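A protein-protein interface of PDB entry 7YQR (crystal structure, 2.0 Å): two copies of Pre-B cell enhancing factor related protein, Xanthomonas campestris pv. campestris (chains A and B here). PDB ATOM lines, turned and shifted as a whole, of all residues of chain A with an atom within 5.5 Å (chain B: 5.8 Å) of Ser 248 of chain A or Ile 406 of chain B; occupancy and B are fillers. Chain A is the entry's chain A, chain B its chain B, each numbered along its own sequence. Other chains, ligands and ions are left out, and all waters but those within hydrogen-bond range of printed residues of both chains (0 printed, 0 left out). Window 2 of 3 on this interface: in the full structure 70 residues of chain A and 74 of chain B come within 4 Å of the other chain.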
ATOM      1  N   HIS A 243      13.126 -21.813   0.611  1.00  0.00           N
ATOM      2  CA  HIS A 243      13.736 -20.641   1.247  1.00  0.00           C
ATOM      3  C   HIS A 243      12.793 -20.021   2.269  1.00  0.00           C
ATOM      4  O   HIS A 243      13.233 -19.586   3.341  1.00  0.00           O
ATOM      5  CB  HIS A 243      14.152 -19.597   0.202  1.00  0.00           C
ATOM      6  CG  HIS A 243      15.224 -18.661   0.682  1.00  0.00           C
ATOM      7  ND1 HIS A 243      16.084 -18.008  -0.176  1.00  0.00           N
ATOM      8  CD2 HIS A 243      15.588 -18.285   1.935  1.00  0.00           C
ATOM      9  CE1 HIS A 243      16.929 -17.271   0.526  1.00  0.00           C
ATOM     10  NE2 HIS A 243      16.650 -17.421   1.810  1.00  0.00           N
ATOM     11  N   SER A 244      11.496 -19.994   1.957  1.00  0.00           N
ATOM     12  CA  SER A 244      10.527 -19.420   2.881  1.00  0.00           C
ATOM     13  C   SER A 244      10.566 -20.127   4.231  1.00  0.00           C
ATOM     14  O   SER A 244      10.586 -19.475   5.284  1.00  0.00           O
ATOM     15  CB  SER A 244       9.124 -19.504   2.283  1.00  0.00           C
ATOM     16  OG  SER A 244       8.573 -20.788   2.510  1.00  0.00           O
ATOM     17  N   THR A 245      10.592 -21.463   4.229  1.00  0.00           N
ATOM     18  CA  THR A 245      10.605 -22.187   5.497  1.00  0.00           C
ATOM     19  C   THR A 245      11.911 -21.973   6.254  1.00  0.00           C
ATOM     20  O   THR A 245      11.910 -21.979   7.491  1.00  0.00           O
ATOM     21  CB  THR A 245      10.318 -23.678   5.263  1.00  0.00           C
ATOM     22  OG1 THR A 245       9.797 -24.241   6.469  1.00  0.00           O
ATOM     23  CG2 THR A 245      11.573 -24.464   4.863  1.00  0.00           C
ATOM     24  N   ILE A 246      13.016 -21.736   5.542  1.00  0.00           N
ATOM     25  CA  ILE A 246      14.243 -21.305   6.208  1.00  0.00           C
ATOM     26  C   ILE A 246      14.006 -19.994   6.952  1.00  0.00           C
ATOM     27  O   ILE A 246      14.283 -19.883   8.150  1.00  0.00           O
ATOM     28  CB  ILE A 246      15.396 -21.177   5.192  1.00  0.00           C
ATOM     29  CG1 ILE A 246      15.774 -22.549   4.626  1.00  0.00           C
ATOM     30  CG2 ILE A 246      16.603 -20.512   5.839  1.00  0.00           C
ATOM     31  CD1 ILE A 246      16.186 -23.556   5.680  1.00  0.00           C
ATOM     32  N   THR A 247      13.480 -18.982   6.254  1.00  0.00           N
ATOM     33  CA  THR A 247      13.308 -17.663   6.865  1.00  0.00           C
ATOM     34  C   THR A 247      12.399 -17.713   8.086  1.00  0.00           C
ATOM     35  O   THR A 247      12.580 -16.930   9.027  1.00  0.00           O
ATOM     36  CB  THR A 247      12.753 -16.670   5.841  1.00  0.00           C
ATOM     37  OG1 THR A 247      11.626 -17.251   5.172  1.00  0.00           O
ATOM     38  CG2 THR A 247      13.813 -16.317   4.809  1.00  0.00           C
ATOM     39  N   SER A 248      11.431 -18.635   8.097  1.00  0.00           N
ATOM     40  CA  SER A 248      10.451 -18.729   9.171  1.00  0.00           C
ATOM     41  C   SER A 248      11.053 -19.133  10.510  1.00  0.00           C
ATOM     42  O   SER A 248      10.374 -19.002  11.536  1.00  0.00           O
ATOM     43  CB  SER A 248       9.357 -19.718   8.782  1.00  0.00           C
ATOM     44  OG  SER A 248       9.630 -20.993   9.325  1.00  0.00           O
ATOM     45  N   TRP A 249      12.290 -19.629  10.538  1.00  0.00           N
ATOM     46  CA  TRP A 249      12.961 -19.801  11.818  1.00  0.00           C
ATOM     47  C   TRP A 249      13.353 -18.467  12.438  1.00  0.00           C
ATOM     48  O   TRP A 249      13.714 -18.436  13.620  1.00  0.00           O
ATOM     49  CB  TRP A 249      14.221 -20.674  11.666  1.00  0.00           C
ATOM     50  CG  TRP A 249      13.975 -22.140  11.357  1.00  0.00           C
ATOM     51  CD1 TRP A 249      13.313 -22.648  10.281  1.00  0.00           C
ATOM     52  CD2 TRP A 249      14.419 -23.273  12.122  1.00  0.00           C
ATOM     53  NE1 TRP A 249      13.300 -24.023  10.332  1.00  0.00           N
ATOM     54  CE2 TRP A 249      13.972 -24.430  11.454  1.00  0.00           C
ATOM     55  CE3 TRP A 249      15.149 -23.422  13.307  1.00  0.00           C
ATOM     56  CZ2 TRP A 249      14.231 -25.719  11.930  1.00  0.00           C
ATOM     57  CZ3 TRP A 249      15.399 -24.697  13.781  1.00  0.00           C
ATOM     58  CH2 TRP A 249      14.942 -25.830  13.095  1.00  0.00           C
ATOM     59  N   GLY A 250      13.298 -17.381  11.678  1.00  0.00           N
ATOM     60  CA  GLY A 250      13.827 -16.111  12.122  1.00  0.00           C
ATOM     61  C   GLY A 250      15.300 -15.960  11.784  1.00  0.00           C
ATOM     62  O   GLY A 250      16.022 -16.929  11.549  1.00  0.00           O
ATOM     63  N   TYR B  36      10.260 -27.205   9.161  1.00  0.00           N
ATOM     64  CA  TYR B  36       9.733 -26.105   9.956  1.00  0.00           C
ATOM     65  C   TYR B  36      10.373 -26.083  11.346  1.00  0.00           C
ATOM     66  O   TYR B  36      10.772 -27.128  11.869  1.00  0.00           O
ATOM     67  CB  TYR B  36       8.216 -26.220  10.094  1.00  0.00           C
ATOM     68  CG  TYR B  36       7.458 -25.805   8.851  1.00  0.00           C
ATOM     69  CD1 TYR B  36       7.139 -24.472   8.622  1.00  0.00           C
ATOM     70  CD2 TYR B  36       7.073 -26.747   7.904  1.00  0.00           C
ATOM     71  CE1 TYR B  36       6.456 -24.082   7.487  1.00  0.00           C
ATOM     72  CE2 TYR B  36       6.390 -26.369   6.761  1.00  0.00           C
ATOM     73  CZ  TYR B  36       6.084 -25.035   6.559  1.00  0.00           C
ATOM     74  OH  TYR B  36       5.402 -24.652   5.431  1.00  0.00           O
ATOM     75  N   PRO B  37      10.457 -24.910  11.973  1.00  0.00           N
ATOM     76  CA  PRO B  37      11.036 -24.823  13.316  1.00  0.00           C
ATOM     77  C   PRO B  37      10.188 -25.581  14.317  1.00  0.00           C
ATOM     78  O   PRO B  37       8.998 -25.829  14.071  1.00  0.00           O
ATOM     79  CB  PRO B  37      11.028 -23.317  13.612  1.00  0.00           C
ATOM     80  CG  PRO B  37       9.932 -22.778  12.788  1.00  0.00           C
ATOM     81  CD  PRO B  37       9.935 -23.607  11.521  1.00  0.00           C
ATOM     82  N   THR B  40       5.989 -25.213  15.523  1.00  0.00           N
ATOM     83  CA  THR B  40       5.129 -24.644  14.488  1.00  0.00           C
ATOM     84  C   THR B  40       3.768 -25.337  14.500  1.00  0.00           C
ATOM     85  O   THR B  40       3.687 -26.569  14.533  1.00  0.00           O
ATOM     86  CB  THR B  40       5.780 -24.786  13.109  1.00  0.00           C
ATOM     87  OG1 THR B  40       7.045 -24.113  13.104  1.00  0.00           O
ATOM     88  CG2 THR B  40       4.883 -24.172  12.023  1.00  0.00           C
ATOM     89  N   CYS B 396       4.760 -17.555   1.585  1.00  0.00           N
ATOM     90  CA  CYS B 396       4.404 -17.677   2.992  1.00  0.00           C
ATOM     91  C   CYS B 396       4.576 -16.315   3.656  1.00  0.00           C
ATOM     92  O   CYS B 396       5.635 -15.691   3.548  1.00  0.00           O
ATOM     93  CB  CYS B 396       5.264 -18.740   3.688  1.00  0.00           C
ATOM     94  SG  CYS B 396       4.897 -18.956   5.441  1.00  0.00           S
ATOM     95  N   SER B 397       3.535 -15.840   4.327  1.00  0.00           N
ATOM     96  CA  SER B 397       3.603 -14.522   4.945  1.00  0.00           C
ATOM     97  C   SER B 397       3.549 -14.569   6.463  1.00  0.00           C
ATOM     98  O   SER B 397       3.822 -13.544   7.098  1.00  0.00           O
ATOM     99  CB  SER B 397       2.471 -13.609   4.447  1.00  0.00           C
ATOM    100  OG  SER B 397       1.202 -14.176   4.724  1.00  0.00           O
ATOM    101  N   ALA B 398       3.203 -15.710   7.060  1.00  0.00           N
ATOM    102  CA  ALA B 398       3.193 -15.820   8.514  1.00  0.00           C
ATOM    103  C   ALA B 398       3.143 -17.288   8.902  1.00  0.00           C
ATOM    104  O   ALA B 398       2.588 -18.118   8.168  1.00  0.00           O
ATOM    105  CB  ALA B 398       2.006 -15.071   9.138  1.00  0.00           C
ATOM    106  N   VAL B 399       3.747 -17.598  10.055  1.00  0.00           N
ATOM    107  CA  VAL B 399       3.605 -18.895  10.707  1.00  0.00           C
ATOM    108  C   VAL B 399       3.313 -18.664  12.182  1.00  0.00           C
ATOM    109  O   VAL B 399       3.659 -17.619  12.741  1.00  0.00           O
ATOM    110  CB  VAL B 399       4.858 -19.784  10.550  1.00  0.00           C
ATOM    111  CG1 VAL B 399       5.042 -20.185   9.107  1.00  0.00           C
ATOM    112  CG2 VAL B 399       6.089 -19.072  11.084  1.00  0.00           C
ATOM    113  N   ARG B 400       2.682 -19.654  12.815  1.00  0.00           N
ATOM    114  CA  ARG B 400       2.440 -19.644  14.254  1.00  0.00           C
ATOM    115  C   ARG B 400       3.373 -20.659  14.912  1.00  0.00           C
ATOM    116  O   ARG B 400       3.368 -21.846  14.552  1.00  0.00           O
ATOM    117  CB  ARG B 400       0.978 -19.954  14.580  1.00  0.00           C
ATOM    118  CG  ARG B 400       0.530 -19.483  15.969  1.00  0.00           C
ATOM    119  CD  ARG B 400      -0.946 -19.782  16.213  1.00  0.00           C
ATOM    120  NE  ARG B 400      -1.252 -21.185  15.955  1.00  0.00           N
ATOM    121  CZ  ARG B 400      -2.482 -21.675  15.820  1.00  0.00           C
ATOM    122  NH1 ARG B 400      -3.532 -20.872  15.922  1.00  0.00           N
ATOM    123  NH2 ARG B 400      -2.665 -22.968  15.579  1.00  0.00           N
ATOM    124  N   VAL B 401       4.173 -20.186  15.860  1.00  0.00           N
ATOM    125  CA  VAL B 401       5.150 -21.004  16.568  1.00  0.00           C
ATOM    126  C   VAL B 401       4.916 -20.814  18.058  1.00  0.00           C
ATOM    127  O   VAL B 401       4.946 -19.680  18.552  1.00  0.00           O
ATOM    128  CB  VAL B 401       6.594 -20.624  16.209  1.00  0.00           C
ATOM    129  CG1 VAL B 401       7.575 -21.422  17.070  1.00  0.00           C
ATOM    130  CG2 VAL B 401       6.856 -20.854  14.726  1.00  0.00           C
ATOM    131  N   ALA B 404       2.217 -18.320  19.030  1.00  0.00           N
ATOM    132  CA  ALA B 404       2.359 -16.926  18.621  1.00  0.00           C
ATOM    133  C   ALA B 404       2.545 -16.809  17.109  1.00  0.00           C
ATOM    134  O   ALA B 404       3.389 -17.500  16.529  1.00  0.00           O
ATOM    135  CB  ALA B 404       3.540 -16.276  19.343  1.00  0.00           C
ATOM    136  N   TRP B 405       1.764 -15.929  16.480  1.00  0.00           N
ATOM    137  CA  TRP B 405       1.951 -15.618  15.066  1.00  0.00           C
ATOM    138  C   TRP B 405       3.183 -14.747  14.872  1.00  0.00           C
ATOM    139  O   TRP B 405       3.427 -13.811  15.637  1.00  0.00           O
ATOM    140  CB  TRP B 405       0.720 -14.898  14.501  1.00  0.00           C
ATOM    141  CG  TRP B 405      -0.406 -15.822  14.195  1.00  0.00           C
ATOM    142  CD1 TRP B 405      -1.516 -16.033  14.953  1.00  0.00           C
ATOM    143  CD2 TRP B 405      -0.527 -16.687  13.052  1.00  0.00           C
ATOM    144  NE1 TRP B 405      -2.323 -16.974  14.360  1.00  0.00           N
ATOM    145  CE2 TRP B 405      -1.740 -17.390  13.190  1.00  0.00           C
ATOM    146  CE3 TRP B 405       0.280 -16.939  11.936  1.00  0.00           C
ATOM    147  CZ2 TRP B 405      -2.178 -18.327  12.245  1.00  0.00           C
ATOM    148  CZ3 TRP B 405      -0.153 -17.875  10.995  1.00  0.00           C
ATOM    149  CH2 TRP B 405      -1.372 -18.555  11.158  1.00  0.00           C
ATOM    150  N   ILE B 406       3.976 -15.061  13.848  1.00  0.00           N
ATOM    151  CA  ILE B 406       5.106 -14.219  13.480  1.00  0.00           C
ATOM    152  C   ILE B 406       5.062 -13.960  11.984  1.00  0.00           C
ATOM    153  O   ILE B 406       4.620 -14.806  11.197  1.00  0.00           O
ATOM    154  CB  ILE B 406       6.478 -14.822  13.886  1.00  0.00           C
ATOM    155  CG1 ILE B 406       6.791 -16.076  13.079  1.00  0.00           C
ATOM    156  CG2 ILE B 406       6.534 -15.108  15.380  1.00  0.00           C
ATOM    157  CD1 ILE B 406       7.856 -16.981  13.712  1.00  0.00           C
ATOM    158  N   ASP B 407       5.505 -12.766  11.602  1.00  0.00           N
ATOM    159  CA  ASP B 407       5.611 -12.400  10.197  1.00  0.00           C
ATOM    160  C   ASP B 407       6.742 -13.182   9.525  1.00  0.00           C
ATOM    161  O   ASP B 407       7.758 -13.489  10.147  1.00  0.00           O
ATOM    162  CB  ASP B 407       5.862 -10.892  10.065  1.00  0.00           C
ATOM    163  CG  ASP B 407       4.661 -10.041  10.491  1.00  0.00           C
ATOM    164  OD1 ASP B 407       3.574 -10.582  10.793  1.00  0.00           O
ATOM    165  OD2 ASP B 407       4.811  -8.806  10.526  1.00  0.00           O
ATOM    166  N   VAL B 408       6.557 -13.498   8.240  1.00  0.00           N
ATOM    167  CA  VAL B 408       7.557 -14.191   7.426  1.00  0.00           C
ATOM    168  C   VAL B 408       7.798 -13.381   6.154  1.00  0.00           C
ATOM    169  O   VAL B 408       6.843 -13.046   5.446  1.00  0.00           O
ATOM    170  CB  VAL B 408       7.119 -15.623   7.052  1.00  0.00           C
ATOM    171  CG1 VAL B 408       8.127 -16.249   6.101  1.00  0.00           C
ATOM    172  CG2 VAL B 408       6.948 -16.484   8.286  1.00  0.00           C
ATOM    173  N   GLY B 423       2.483 -11.059   7.339  1.00  0.00           N
ATOM    174  CA  GLY B 423       1.409 -11.273   8.277  1.00  0.00           C
ATOM    175  C   GLY B 423       0.208 -11.921   7.614  1.00  0.00           C
ATOM    176  O   GLY B 423       0.242 -12.353   6.453  1.00  0.00           O
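No position is printed for both chains.
Among the printed residues, pairs that only touch across the chains: Thr 245 of chain A with Tyr 36 of chain B (3.4 Å), Thr 247 of chain A with Val 408 of chain B (3.8 Å), Ser 248 of chain A with Pro 37 of chain B (3.4 Å), Ser 248 of chain A with Ile 406 of chain B (3.9 Å) and Trp 249 of chain A with Tyr 36 of chain B (3.7 Å).
Ser 244 of chain A touches none of the printed residues of chain B. Printed residues of chain B within 4 Å of Thr 247 of chain A: Val 408 (3.8 Å). Printed residues of chain B within 4 Å of Trp 249 of chain A: Tyr 36 and Pro 37. Printed residues of chain A within 4 Å of Tyr 36 of chain B: Thr 245 and Trp 249. Val 399 of chain B touches none of the printed residues of chain A. Of chain A, only Ser 248 comes within 4 Å of Ile 406 of chain B. Printed residues of chain A within 4 Å of Val 408 of chain B: Thr 247 (3.8 Å). The nearest printed residue of chain B that does not touch Ser 248 of chain A is Val 399 of chain B (4.05 Å). The nearest printed residue of chain A that does not touch Ile 406 of chain B is Gly 250 of chain A (5.8 Å).
Hydrophobic or aromatic side chains of chain A within 4 Å of the printed part of chain B: Trp 249. Of the 15 printed residues of chain B, 4 touch a printed residue of chain A. Hydrophobic or aromatic side chains of chain B that line the printed part of chain A: Tyr 36, Pro 37, Ile 406 and Val 408. Along chain B the printed residues that touch a printed residue of chain A span positions 36 to 408. Among the printed residues, no Asp or Glu carboxylate lies within 4 Å of a Lys or Arg side-chain nitrogen of the other chain.
OG1 of Thr 247 of chain A lies within hydrogen-bond range of O of Ser 244 of chain A (2.5 Å). O of His 243 of chain A is in hydrogen-bond range of OG1 of Thr 247 of chain A (3.4 Å). O of Thr 245 of chain A is in hydrogen-bond range of OG of Ser 248 of chain A (3.1 Å). OG1 of Thr 40 of chain B is in hydrogen-bond range of O of Pro 37 of chain B (2.8 Å). The backbone carbonyl oxygen (O) of Val 399 of chain B is in hydrogen-bond range of the backbone NH (N) of Ile 406 of chain B, at 2.8 Å. The backbone carbonyl oxygen (O) of Ser 397 of chain B is in hydrogen-bond range of the backbone NH (N) of Val 408 of chain B, 3.0 Å away.
The indole nitrogen (NE1) of Trp 249 of chain A sits close to the backbone nitrogen (N) of Pro 37 of chain B (3.4 Å).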
